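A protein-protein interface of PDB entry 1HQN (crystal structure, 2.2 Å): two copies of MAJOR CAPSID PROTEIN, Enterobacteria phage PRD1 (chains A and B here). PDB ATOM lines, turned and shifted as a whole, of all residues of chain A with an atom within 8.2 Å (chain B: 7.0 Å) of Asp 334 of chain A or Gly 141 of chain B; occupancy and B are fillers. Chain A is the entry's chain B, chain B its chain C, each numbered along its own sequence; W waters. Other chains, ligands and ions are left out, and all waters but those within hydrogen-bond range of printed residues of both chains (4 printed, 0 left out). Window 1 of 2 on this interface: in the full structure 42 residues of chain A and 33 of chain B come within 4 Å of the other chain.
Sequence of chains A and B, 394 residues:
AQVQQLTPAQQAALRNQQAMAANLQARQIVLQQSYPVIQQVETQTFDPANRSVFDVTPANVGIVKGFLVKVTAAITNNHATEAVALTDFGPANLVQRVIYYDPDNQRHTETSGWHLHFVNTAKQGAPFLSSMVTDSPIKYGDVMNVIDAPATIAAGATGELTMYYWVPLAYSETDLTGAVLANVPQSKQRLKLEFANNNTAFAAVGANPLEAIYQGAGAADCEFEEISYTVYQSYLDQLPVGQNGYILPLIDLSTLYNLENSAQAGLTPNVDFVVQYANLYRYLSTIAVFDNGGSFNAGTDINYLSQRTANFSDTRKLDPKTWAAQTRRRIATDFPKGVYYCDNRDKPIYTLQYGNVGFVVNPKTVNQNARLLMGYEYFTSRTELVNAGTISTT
NH2 of Arg 328 of chain A sits close to N of Asn 145 of chain B, at 3.4 Å. The backbone NH (N) of Val 143 of chain B sits at hydrogen-bond distance from the side-chain carboxylate (OD2) of Asp 334 of chain A (2.8 Å). The backbone carbonyl oxygen (O) of Ala 332 of chain A sits close to the backbone carbonyl oxygen (O) of Ser 130 of chain B, 3.3 Å away. N of Val 146 of chain B sits close to NH2 of Arg 328 of chain A (3.4 Å). The side-chain sulfur of Met 144 of chain B lies close to the backbone carbonyl oxygen of Ala 298 of chain A (3.5 Å). O of Ala 332 of chain A lies within hydrogen-bond range of N of Met 132 of chain B. NH2 of Arg 328 of chain A is in salt-bridge range of OD1 of Asp 142 of chain B (3.1 Å). The side-chain carboxylate (OD2) of Asp 334 of chain A is in hydrogen-bond range of the backbone NH (N) of Met 144 of chain B, 2.7 Å away. O of Leu 129 of chain B lies within hydrogen-bond range of NH1 of Arg 328 of chain A (2.9 Å). The side-chain hydroxyl (OG1) of Thr 121 of chain A is in hydrogen-bond range of the side-chain hydroxyl (OH) of Tyr 140 of chain B (2.6 Å). OG1 of Thr 333 of chain A is in hydrogen-bond range of OG of Ser 131 of chain B (2.6 Å). The backbone NH (N) of Asp 334 of chain A sits close to the backbone carbonyl oxygen (O) of Gly 141 of chain B (3.4 Å). NZ of Lys 321 of chain A lies within hydrogen-bond range of O of Asn 145 of chain B (2.9 Å). The side-chain hydroxyl (OG1) of Thr 333 of chain A lies within hydrogen-bond range of the backbone NH (N) of Gly 141 of chain B (3.2 Å).
The side-chain carboxylate (OD2) of Asp 142 of chain B sits close to the side-chain amide oxygen (OD1) of Asn 145 of chain B (2.8 Å).
Of the printed residues of chain B, Lys 321 of chain A touches Met 144, Asn 145 and Val 146. Of the printed residues of chain B, Asp 334 of chain A touches Tyr 140, Gly 141, Asp 142, Val 143, Met 144 and Asn 145. Gly 141 of chain B touches two residues of chain A. The nearest printed residue of chain B that does not touch Ala 324 of chain A is Leu 129 of chain B (6.3 Å).
Of the 14 printed residues of chain B, 13 touch a printed residue of chain A. Hydrophobic or aromatic side chains of chain B that line the printed part of chain A: Leu 129, Met 132, Ile 138, Tyr 140, Val 143, Met 144 and Val 146. Among the printed residues, Asp or Glu carboxylates within 4 Å of a Lys or Arg side-chain nitrogen of the other chain: Arg 328 of chain A with Asp 142 of chain B.
No position is printed for both chains. Of the 37 pairs that touch across the chains among the printed residues, none has its exchanged pair printed and touching as well.
Water W1 lies within hydrogen-bond range of O of Met 132 of chain B (2.7 Å), OG1 of Thr 333 of chain A (2.7 Å) and N of Gly 141 of chain B (3.4 Å). Water W2 lies within hydrogen-bond range of O of Ser 130 of chain B and O of Arg 328 of chain A.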
ATOM      1  N   PHE A 118     -18.954  36.597 -28.194  1.00  0.00           N
ATOM      2  CA  PHE A 118     -20.004  35.591 -28.352  1.00  0.00           C
ATOM      3  C   PHE A 118     -19.949  34.993 -29.759  1.00  0.00           C
ATOM      4  O   PHE A 118     -20.196  33.805 -29.937  1.00  0.00           O
ATOM      5  CB  PHE A 118     -21.379  36.195 -28.048  1.00  0.00           C
ATOM      6  CG  PHE A 118     -21.607  36.472 -26.577  1.00  0.00           C
ATOM      7  CD1 PHE A 118     -20.960  35.712 -25.602  1.00  0.00           C
ATOM      8  CD2 PHE A 118     -22.465  37.487 -26.168  1.00  0.00           C
ATOM      9  CE1 PHE A 118     -21.163  35.959 -24.233  1.00  0.00           C
ATOM     10  CE2 PHE A 118     -22.679  37.746 -24.804  1.00  0.00           C
ATOM     11  CZ  PHE A 118     -22.023  36.978 -23.834  1.00  0.00           C
ATOM     12  N   THR A 121     -17.166  32.497 -29.994  1.00  0.00           N
ATOM     13  CA  THR A 121     -17.667  31.258 -29.398  1.00  0.00           C
ATOM     14  C   THR A 121     -18.570  30.500 -30.379  1.00  0.00           C
ATOM     15  O   THR A 121     -18.400  29.295 -30.609  1.00  0.00           O
ATOM     16  CB  THR A 121     -18.475  31.555 -28.114  1.00  0.00           C
ATOM     17  OG1 THR A 121     -17.575  31.904 -27.055  1.00  0.00           O
ATOM     18  CG2 THR A 121     -19.316  30.354 -27.706  1.00  0.00           C
ATOM     19  N   PRO A 127     -17.198  27.476 -26.060  1.00  0.00           N
ATOM     20  CA  PRO A 127     -16.661  28.709 -25.462  1.00  0.00           C
ATOM     21  C   PRO A 127     -15.273  28.992 -26.037  1.00  0.00           C
ATOM     22  O   PRO A 127     -14.375  28.161 -25.941  1.00  0.00           O
ATOM     23  CB  PRO A 127     -16.632  28.375 -23.972  1.00  0.00           C
ATOM     24  CG  PRO A 127     -17.902  27.590 -23.821  1.00  0.00           C
ATOM     25  CD  PRO A 127     -17.800  26.616 -25.023  1.00  0.00           C
ATOM     26  N   ALA A 298     -32.580  33.759 -16.729  1.00  0.00           N
ATOM     27  CA  ALA A 298     -32.459  32.525 -17.507  1.00  0.00           C
ATOM     28  C   ALA A 298     -33.789  32.156 -18.181  1.00  0.00           C
ATOM     29  O   ALA A 298     -34.426  31.161 -17.817  1.00  0.00           O
ATOM     30  CB  ALA A 298     -31.999  31.382 -16.604  1.00  0.00           C
ATOM     31  N   PRO A 320     -38.396  29.734 -24.493  1.00  0.00           N
ATOM     32  CA  PRO A 320     -36.985  29.913 -24.125  1.00  0.00           C
ATOM     33  C   PRO A 320     -36.121  28.652 -24.026  1.00  0.00           C
ATOM     34  O   PRO A 320     -35.019  28.623 -24.567  1.00  0.00           O
ATOM     35  CB  PRO A 320     -37.071  30.668 -22.804  1.00  0.00           C
ATOM     36  CG  PRO A 320     -38.314  31.509 -22.995  1.00  0.00           C
ATOM     37  CD  PRO A 320     -39.274  30.495 -23.586  1.00  0.00           C
ATOM     38  N   LYS A 321     -36.600  27.611 -23.353  1.00  0.00           N
ATOM     39  CA  LYS A 321     -35.787  26.404 -23.228  1.00  0.00           C
ATOM     40  C   LYS A 321     -35.553  25.673 -24.544  1.00  0.00           C
ATOM     41  O   LYS A 321     -34.453  25.184 -24.796  1.00  0.00           O
ATOM     42  CB  LYS A 321     -36.382  25.440 -22.203  1.00  0.00           C
ATOM     43  CG  LYS A 321     -36.091  25.822 -20.753  1.00  0.00           C
ATOM     44  CD  LYS A 321     -36.309  24.633 -19.811  1.00  0.00           C
ATOM     45  CE  LYS A 321     -35.961  24.987 -18.371  1.00  0.00           C
ATOM     46  NZ  LYS A 321     -35.862  23.775 -17.502  1.00  0.00           N
ATOM     47  N   TRP A 323     -35.578  27.061 -27.429  1.00  0.00           N
ATOM     48  CA  TRP A 323     -34.707  27.949 -28.186  1.00  0.00           C
ATOM     49  C   TRP A 323     -33.266  27.649 -27.717  1.00  0.00           C
ATOM     50  O   TRP A 323     -32.357  27.452 -28.529  1.00  0.00           O
ATOM     51  CB  TRP A 323     -35.085  29.407 -27.898  1.00  0.00           C
ATOM     52  CG  TRP A 323     -34.292  30.409 -28.674  1.00  0.00           C
ATOM     53  CD1 TRP A 323     -33.024  30.841 -28.401  1.00  0.00           C
ATOM     54  CD2 TRP A 323     -34.695  31.078 -29.879  1.00  0.00           C
ATOM     55  NE1 TRP A 323     -32.613  31.734 -29.357  1.00  0.00           N
ATOM     56  CE2 TRP A 323     -33.617  31.898 -30.279  1.00  0.00           C
ATOM     57  CE3 TRP A 323     -35.859  31.058 -30.665  1.00  0.00           C
ATOM     58  CZ2 TRP A 323     -33.665  32.698 -31.431  1.00  0.00           C
ATOM     59  CZ3 TRP A 323     -35.911  31.849 -31.814  1.00  0.00           C
ATOM     60  CH2 TRP A 323     -34.814  32.660 -32.184  1.00  0.00           C
ATOM     61  N   ALA A 324     -33.077  27.581 -26.400  1.00  0.00           N
ATOM     62  CA  ALA A 324     -31.767  27.296 -25.817  1.00  0.00           C
ATOM     63  C   ALA A 324     -31.245  25.939 -26.281  1.00  0.00           C
ATOM     64  O   ALA A 324     -30.045  25.769 -26.485  1.00  0.00           O
ATOM     65  CB  ALA A 324     -31.847  27.318 -24.293  1.00  0.00           C
ATOM     66  N   ALA A 325     -32.141  24.967 -26.417  1.00  0.00           N
ATOM     67  CA  ALA A 325     -31.754  23.637 -26.873  1.00  0.00           C
ATOM     68  C   ALA A 325     -31.069  23.743 -28.242  1.00  0.00           C
ATOM     69  O   ALA A 325     -30.043  23.099 -28.502  1.00  0.00           O
ATOM     70  CB  ALA A 325     -32.988  22.740 -26.974  1.00  0.00           C
ATOM     71  N   GLN A 326     -31.641  24.574 -29.109  1.00  0.00           N
ATOM     72  CA  GLN A 326     -31.104  24.770 -30.450  1.00  0.00           C
ATOM     73  C   GLN A 326     -29.665  25.282 -30.369  1.00  0.00           C
ATOM     74  O   GLN A 326     -28.799  24.859 -31.141  1.00  0.00           O
ATOM     75  CB  GLN A 326     -31.976  25.769 -31.212  1.00  0.00           C
ATOM     76  CG  GLN A 326     -32.415  25.302 -32.578  1.00  0.00           C
ATOM     77  CD  GLN A 326     -33.118  23.949 -32.544  1.00  0.00           C
ATOM     78  OE1 GLN A 326     -32.563  22.936 -32.972  1.00  0.00           O
ATOM     79  NE2 GLN A 326     -34.342  23.928 -32.024  1.00  0.00           N
ATOM     80  N   THR A 327     -29.424  26.183 -29.421  1.00  0.00           N
ATOM     81  CA  THR A 327     -28.101  26.765 -29.205  1.00  0.00           C
ATOM     82  C   THR A 327     -27.115  25.727 -28.645  1.00  0.00           C
ATOM     83  O   THR A 327     -25.940  25.697 -29.044  1.00  0.00           O
ATOM     84  CB  THR A 327     -28.195  27.989 -28.259  1.00  0.00           C
ATOM     85  OG1 THR A 327     -28.864  29.057 -28.943  1.00  0.00           O
ATOM     86  CG2 THR A 327     -26.814  28.459 -27.826  1.00  0.00           C
ATOM     87  N   ARG A 328     -27.592  24.879 -27.735  1.00  0.00           N
ATOM     88  CA  ARG A 328     -26.745  23.830 -27.174  1.00  0.00           C
ATOM     89  C   ARG A 328     -26.180  22.931 -28.277  1.00  0.00           C
ATOM     90  O   ARG A 328     -25.103  22.373 -28.135  1.00  0.00           O
ATOM     91  CB  ARG A 328     -27.521  22.987 -26.159  1.00  0.00           C
ATOM     92  CG  ARG A 328     -27.772  23.722 -24.839  1.00  0.00           C
ATOM     93  CD  ARG A 328     -28.025  22.743 -23.683  1.00  0.00           C
ATOM     94  NE  ARG A 328     -28.223  23.435 -22.408  1.00  0.00           N
ATOM     95  CZ  ARG A 328     -28.242  22.837 -21.220  1.00  0.00           C
ATOM     96  NH1 ARG A 328     -28.077  21.514 -21.123  1.00  0.00           N
ATOM     97  NH2 ARG A 328     -28.414  23.564 -20.122  1.00  0.00           N
ATOM     98  N   ARG A 329     -26.913  22.796 -29.378  1.00  0.00           N
ATOM     99  CA  ARG A 329     -26.448  21.986 -30.501  1.00  0.00           C
ATOM    100  C   ARG A 329     -25.339  22.744 -31.234  1.00  0.00           C
ATOM    101  O   ARG A 329     -24.510  22.149 -31.914  1.00  0.00           O
ATOM    102  CB  ARG A 329     -27.589  21.734 -31.483  1.00  0.00           C
ATOM    103  CG  ARG A 329     -28.759  20.998 -30.894  1.00  0.00           C
ATOM    104  CD  ARG A 329     -28.483  19.510 -30.838  1.00  0.00           C
ATOM    105  NE  ARG A 329     -28.368  18.959 -32.181  1.00  0.00           N
ATOM    106  CZ  ARG A 329     -28.269  17.661 -32.455  1.00  0.00           C
ATOM    107  NH1 ARG A 329     -28.271  16.767 -31.476  1.00  0.00           N
ATOM    108  NH2 ARG A 329     -28.173  17.258 -33.717  1.00  0.00           N
ATOM    109  N   ILE A 331     -23.104  25.378 -29.690  1.00  0.00           N
ATOM    110  CA  ILE A 331     -21.893  25.618 -28.901  1.00  0.00           C
ATOM    111  C   ILE A 331     -21.705  24.701 -27.693  1.00  0.00           C
ATOM    112  O   ILE A 331     -20.943  25.026 -26.781  1.00  0.00           O
ATOM    113  CB  ILE A 331     -21.831  27.093 -28.402  1.00  0.00           C
ATOM    114  CG1 ILE A 331     -22.941  27.353 -27.386  1.00  0.00           C
ATOM    115  CG2 ILE A 331     -21.983  28.055 -29.584  1.00  0.00           C
ATOM    116  CD1 ILE A 331     -22.883  28.743 -26.757  1.00  0.00           C
ATOM    117  N   ALA A 332     -22.420  23.577 -27.680  1.00  0.00           N
ATOM    118  CA  ALA A 332     -22.314  22.588 -26.616  1.00  0.00           C
ATOM    119  C   ALA A 332     -22.612  23.069 -25.193  1.00  0.00           C
ATOM    120  O   ALA A 332     -22.229  22.406 -24.224  1.00  0.00           O
ATOM    121  CB  ALA A 332     -20.916  21.947 -26.660  1.00  0.00           C
ATOM    122  N   THR A 333     -23.283  24.211 -25.059  1.00  0.00           N
ATOM    123  CA  THR A 333     -23.619  24.754 -23.746  1.00  0.00           C
ATOM    124  C   THR A 333     -24.555  25.964 -23.941  1.00  0.00           C
ATOM    125  O   THR A 333     -24.987  26.236 -25.060  1.00  0.00           O
ATOM    126  CB  THR A 333     -22.319  25.151 -22.991  1.00  0.00           C
ATOM    127  OG1 THR A 333     -22.626  25.505 -21.637  1.00  0.00           O
ATOM    128  CG2 THR A 333     -21.600  26.306 -23.703  1.00  0.00           C
ATOM    129  N   ASP A 334     -24.891  26.676 -22.869  1.00  0.00           N
ATOM    130  CA  ASP A 334     -25.766  27.847 -23.000  1.00  0.00           C
ATOM    131  C   ASP A 334     -24.925  29.113 -22.944  1.00  0.00           C
ATOM    132  O   ASP A 334     -23.870  29.136 -22.301  1.00  0.00           O
ATOM    133  CB  ASP A 334     -26.772  27.957 -21.834  1.00  0.00           C
ATOM    134  CG  ASP A 334     -27.642  26.718 -21.658  1.00  0.00           C
ATOM    135  OD1 ASP A 334     -28.055  26.110 -22.661  1.00  0.00           O
ATOM    136  OD2 ASP A 334     -27.930  26.376 -20.492  1.00  0.00           O
ATOM    137  N   PHE A 335     -25.397  30.165 -23.607  1.00  0.00           N
ATOM    138  CA  PHE A 335     -24.732  31.458 -23.532  1.00  0.00           C
ATOM    139  C   PHE A 335     -25.134  31.991 -22.145  1.00  0.00           C
ATOM    140  O   PHE A 335     -26.053  31.466 -21.516  1.00  0.00           O
ATOM    141  CB  PHE A 335     -25.247  32.410 -24.620  1.00  0.00           C
ATOM    142  CG  PHE A 335     -24.525  32.285 -25.925  1.00  0.00           C
ATOM    143  CD1 PHE A 335     -23.262  32.861 -26.091  1.00  0.00           C
ATOM    144  CD2 PHE A 335     -25.089  31.584 -26.986  1.00  0.00           C
ATOM    145  CE1 PHE A 335     -22.570  32.744 -27.299  1.00  0.00           C
ATOM    146  CE2 PHE A 335     -24.408  31.457 -28.198  1.00  0.00           C
ATOM    147  CZ  PHE A 335     -23.138  32.043 -28.356  1.00  0.00           C
ATOM    148  N   PRO A 336     -24.447  33.022 -21.642  1.00  0.00           N
ATOM    149  CA  PRO A 336     -24.801  33.559 -20.323  1.00  0.00           C
ATOM    150  C   PRO A 336     -26.277  33.977 -20.207  1.00  0.00           C
ATOM    151  O   PRO A 336     -26.984  34.114 -21.220  1.00  0.00           O
ATOM    152  CB  PRO A 336     -23.842  34.732 -20.174  1.00  0.00           C
ATOM    153  CG  PRO A 336     -22.617  34.214 -20.861  1.00  0.00           C
ATOM    154  CD  PRO A 336     -23.198  33.625 -22.130  1.00  0.00           C
ATOM    155  N   LYS A 337     -26.726  34.170 -18.968  1.00  0.00           N
ATOM    156  CA  LYS A 337     -28.108  34.540 -18.692  1.00  0.00           C
ATOM    157  C   LYS A 337     -28.587  35.738 -19.513  1.00  0.00           C
ATOM    158  O   LYS A 337     -27.915  36.779 -19.570  1.00  0.00           O
ATOM    159  CB  LYS A 337     -28.299  34.866 -17.204  1.00  0.00           C
ATOM    160  CG  LYS A 337     -28.055  33.710 -16.258  1.00  0.00           C
ATOM    161  CD  LYS A 337     -28.501  34.067 -14.850  1.00  0.00           C
ATOM    162  CE  LYS A 337     -27.773  35.303 -14.353  1.00  0.00           C
ATOM    163  NZ  LYS A 337     -28.338  35.800 -13.072  1.00  0.00           N
ATOM    164  N   VAL A 339     -28.830  35.962 -22.706  1.00  0.00           N
ATOM    165  CA  VAL A 339     -28.251  36.018 -24.045  1.00  0.00           C
ATOM    166  C   VAL A 339     -28.864  34.937 -24.936  1.00  0.00           C
ATOM    167  O   VAL A 339     -28.823  33.753 -24.590  1.00  0.00           O
ATOM    168  CB  VAL A 339     -26.713  35.809 -24.000  1.00  0.00           C
ATOM    169  CG1 VAL A 339     -26.120  35.944 -25.403  1.00  0.00           C
ATOM    170  CG2 VAL A 339     -26.080  36.812 -23.029  1.00  0.00           C
ATOM    171  N   TYR A 341     -29.080  33.245 -28.884  1.00  0.00           N
ATOM    172  CA  TYR A 341     -28.416  33.112 -30.161  1.00  0.00           C
ATOM    173  C   TYR A 341     -29.311  32.468 -31.205  1.00  0.00           C
ATOM    174  O   TYR A 341     -30.145  31.618 -30.890  1.00  0.00           O
ATOM    175  CB  TYR A 341     -27.150  32.267 -29.970  1.00  0.00           C
ATOM    176  CG  TYR A 341     -26.381  31.967 -31.235  1.00  0.00           C
ATOM    177  CD1 TYR A 341     -25.688  32.971 -31.909  1.00  0.00           C
ATOM    178  CD2 TYR A 341     -26.331  30.667 -31.751  1.00  0.00           C
ATOM    179  CE1 TYR A 341     -24.958  32.692 -33.069  1.00  0.00           C
ATOM    180  CE2 TYR A 341     -25.604  30.376 -32.912  1.00  0.00           C
ATOM    181  CZ  TYR A 341     -24.922  31.395 -33.562  1.00  0.00           C
ATOM    182  OH  TYR A 341     -24.193  31.120 -34.692  1.00  0.00           O
ATOM    183  N   LEU B 129     -28.111  17.336 -26.147  1.00  0.00           N
ATOM    184  CA  LEU B 129     -28.408  18.662 -25.598  1.00  0.00           C
ATOM    185  C   LEU B 129     -27.768  18.943 -24.241  1.00  0.00           C
ATOM    186  O   LEU B 129     -28.304  19.717 -23.447  1.00  0.00           O
ATOM    187  CB  LEU B 129     -29.930  18.861 -25.486  1.00  0.00           C
ATOM    188  CG  LEU B 129     -30.740  18.719 -26.783  1.00  0.00           C
ATOM    189  CD1 LEU B 129     -32.204  19.060 -26.504  1.00  0.00           C
ATOM    190  CD2 LEU B 129     -30.177  19.652 -27.850  1.00  0.00           C
ATOM    191  N   SER B 130     -26.626  18.322 -23.963  1.00  0.00           N
ATOM    192  CA  SER B 130     -25.966  18.561 -22.684  1.00  0.00           C
ATOM    193  C   SER B 130     -25.133  19.844 -22.733  1.00  0.00           C
ATOM    194  O   SER B 130     -24.876  20.402 -23.804  1.00  0.00           O
ATOM    195  CB  SER B 130     -25.048  17.386 -22.329  1.00  0.00           C
ATOM    196  OG  SER B 130     -24.011  17.248 -23.290  1.00  0.00           O
ATOM    197  N   SER B 131     -24.729  20.304 -21.553  1.00  0.00           N
ATOM    198  CA  SER B 131     -23.893  21.482 -21.412  1.00  0.00           C
ATOM    199  C   SER B 131     -22.531  20.995 -20.924  1.00  0.00           C
ATOM    200  O   SER B 131     -22.398  20.477 -19.813  1.00  0.00           O
ATOM    201  CB  SER B 131     -24.484  22.457 -20.390  1.00  0.00           C
ATOM    202  OG  SER B 131     -23.602  23.548 -20.164  1.00  0.00           O
ATOM    203  N   MET B 132     -21.536  21.151 -21.784  1.00  0.00           N
ATOM    204  CA  MET B 132     -20.151  20.767 -21.521  1.00  0.00           C
ATOM    205  C   MET B 132     -19.528  21.707 -20.481  1.00  0.00           C
ATOM    206  O   MET B 132     -19.797  22.908 -20.487  1.00  0.00           O
ATOM    207  CB  MET B 132     -19.386  20.850 -22.846  1.00  0.00           C
ATOM    208  CG  MET B 132     -17.886  20.615 -22.800  1.00  0.00           C
ATOM    209  SD  MET B 132     -17.126  20.993 -24.573  1.00  0.00           S
ATOM    210  CE  MET B 132     -17.602  22.843 -24.702  1.00  0.00           C
ATOM    211  N   VAL B 133     -18.705  21.164 -19.589  1.00  0.00           N
ATOM    212  CA  VAL B 133     -18.041  21.963 -18.553  1.00  0.00           C
ATOM    213  C   VAL B 133     -16.663  22.418 -19.054  1.00  0.00           C
ATOM    214  O   VAL B 133     -15.927  21.623 -19.631  1.00  0.00           O
ATOM    215  CB  VAL B 133     -17.846  21.135 -17.253  1.00  0.00           C
ATOM    216  CG1 VAL B 133     -17.020  21.926 -16.229  1.00  0.00           C
ATOM    217  CG2 VAL B 133     -19.202  20.778 -16.657  1.00  0.00           C
ATOM    218  N   ILE B 138     -16.092  33.395 -18.472  1.00  0.00           N
ATOM    219  CA  ILE B 138     -17.364  33.958 -18.941  1.00  0.00           C
ATOM    220  C   ILE B 138     -18.388  32.921 -18.486  1.00  0.00           C
ATOM    221  O   ILE B 138     -18.176  31.706 -18.654  1.00  0.00           O
ATOM    222  CB  ILE B 138     -17.415  34.093 -20.486  1.00  0.00           C
ATOM    223  CG1 ILE B 138     -16.457  35.190 -20.949  1.00  0.00           C
ATOM    224  CG2 ILE B 138     -18.813  34.403 -20.945  1.00  0.00           C
ATOM    225  CD1 ILE B 138     -15.049  34.709 -21.138  1.00  0.00           C
ATOM    226  N   LYS B 139     -19.507  33.386 -17.942  1.00  0.00           N
ATOM    227  CA  LYS B 139     -20.491  32.464 -17.386  1.00  0.00           C
ATOM    228  C   LYS B 139     -21.388  31.602 -18.280  1.00  0.00           C
ATOM    229  O   LYS B 139     -22.621  31.617 -18.155  1.00  0.00           O
ATOM    230  CB  LYS B 139     -21.338  33.194 -16.337  1.00  0.00           C
ATOM    231  CG  LYS B 139     -20.496  33.857 -15.224  1.00  0.00           C
ATOM    232  CD  LYS B 139     -21.234  33.855 -13.887  1.00  0.00           C
ATOM    233  CE  LYS B 139     -20.646  34.850 -12.901  1.00  0.00           C
ATOM    234  NZ  LYS B 139     -19.225  34.611 -12.603  1.00  0.00           N
ATOM    235  N   TYR B 140     -20.753  30.854 -19.182  1.00  0.00           N
ATOM    236  CA  TYR B 140     -21.467  29.893 -20.018  1.00  0.00           C
ATOM    237  C   TYR B 140     -21.717  28.801 -18.992  1.00  0.00           C
ATOM    238  O   TYR B 140     -21.195  28.873 -17.875  1.00  0.00           O
ATOM    239  CB  TYR B 140     -20.569  29.280 -21.096  1.00  0.00           C
ATOM    240  CG  TYR B 140     -20.099  30.243 -22.144  1.00  0.00           C
ATOM    241  CD1 TYR B 140     -20.896  30.523 -23.253  1.00  0.00           C
ATOM    242  CD2 TYR B 140     -18.865  30.890 -22.028  1.00  0.00           C
ATOM    243  CE1 TYR B 140     -20.479  31.421 -24.227  1.00  0.00           C
ATOM    244  CE2 TYR B 140     -18.435  31.797 -23.005  1.00  0.00           C
ATOM    245  CZ  TYR B 140     -19.253  32.051 -24.099  1.00  0.00           C
ATOM    246  OH  TYR B 140     -18.857  32.916 -25.075  1.00  0.00           O
ATOM    247  N   GLY B 141     -22.484  27.786 -19.366  1.00  0.00           N
ATOM    248  CA  GLY B 141     -22.723  26.689 -18.446  1.00  0.00           C
ATOM    249  C   GLY B 141     -24.158  26.232 -18.497  1.00  0.00           C
ATOM    250  O   GLY B 141     -24.868  26.508 -19.466  1.00  0.00           O
ATOM    251  N   ASP B 142     -24.576  25.510 -17.464  1.00  0.00           N
ATOM    252  CA  ASP B 142     -25.946  25.040 -17.392  1.00  0.00           C
ATOM    253  C   ASP B 142     -26.762  26.235 -16.916  1.00  0.00           C
ATOM    254  O   ASP B 142     -27.025  26.403 -15.726  1.00  0.00           O
ATOM    255  CB  ASP B 142     -26.058  23.868 -16.412  1.00  0.00           C
ATOM    256  CG  ASP B 142     -27.485  23.399 -16.227  1.00  0.00           C
ATOM    257  OD1 ASP B 142     -28.365  23.828 -17.004  1.00  0.00           O
ATOM    258  OD2 ASP B 142     -27.722  22.595 -15.303  1.00  0.00           O
ATOM    259  N   VAL B 143     -27.141  27.072 -17.871  1.00  0.00           N
ATOM    260  CA  VAL B 143     -27.903  28.282 -17.597  1.00  0.00           C
ATOM    261  C   VAL B 143     -29.403  28.073 -17.765  1.00  0.00           C
ATOM    262  O   VAL B 143     -30.196  28.479 -16.913  1.00  0.00           O
ATOM    263  CB  VAL B 143     -27.454  29.428 -18.553  1.00  0.00           C
ATOM    264  CG1 VAL B 143     -28.359  30.644 -18.393  1.00  0.00           C
ATOM    265  CG2 VAL B 143     -25.987  29.793 -18.287  1.00  0.00           C
ATOM    266  N   MET B 144     -29.774  27.429 -18.869  1.00  0.00           N
ATOM    267  CA  MET B 144     -31.165  27.194 -19.227  1.00  0.00           C
ATOM    268  C   MET B 144     -31.743  25.840 -18.838  1.00  0.00           C
ATOM    269  O   MET B 144     -32.914  25.568 -19.103  1.00  0.00           O
ATOM    270  CB  MET B 144     -31.332  27.383 -20.738  1.00  0.00           C
ATOM    271  CG  MET B 144     -31.125  28.801 -21.232  1.00  0.00           C
ATOM    272  SD  MET B 144     -32.404  30.042 -20.469  1.00  0.00           S
ATOM    273  CE  MET B 144     -34.054  29.205 -21.073  1.00  0.00           C
ATOM    274  N   ASN B 145     -30.923  24.985 -18.238  1.00  0.00           N
ATOM    275  CA  ASN B 145     -31.385  23.667 -17.821  1.00  0.00           C
ATOM    276  C   ASN B 145     -32.275  22.974 -18.853  1.00  0.00           C
ATOM    277  O   ASN B 145     -33.418  22.612 -18.553  1.00  0.00           O
ATOM    278  CB  ASN B 145     -32.134  23.792 -16.492  1.00  0.00           C
ATOM    279  CG  ASN B 145     -31.193  24.036 -15.327  1.00  0.00           C
ATOM    280  OD1 ASN B 145     -30.430  23.140 -14.921  1.00  0.00           O
ATOM    281  ND2 ASN B 145     -31.221  25.250 -14.796  1.00  0.00           N
ATOM    282  N   VAL B 146     -31.742  22.788 -20.060  1.00  0.00           N
ATOM    283  CA  VAL B 146     -32.487  22.147 -21.143  1.00  0.00           C
ATOM    284  C   VAL B 146     -32.897  20.712 -20.787  1.00  0.00           C
ATOM    285  O   VAL B 146     -34.068  20.379 -20.933  1.00  0.00           O
ATOM    286  CB  VAL B 146     -31.696  22.209 -22.451  1.00  0.00           C
ATOM    287  CG1 VAL B 146     -32.474  21.532 -23.568  1.00  0.00           C
ATOM    288  CG2 VAL B 146     -31.448  23.666 -22.798  1.00  0.00           C
HETATM  289  O   HOH W   1     -20.151  25.591 -20.464  1.00  0.00           O
HETATM  290  O   HOH W   2     -25.597  20.010 -26.408  1.00  0.00           O
HETATM  291  O   HOH W   3     -24.759  33.132 -16.947  1.00  0.00           O
HETATM  292  O   HOH W   4     -22.160  19.228 -24.449  1.00  0.00           O
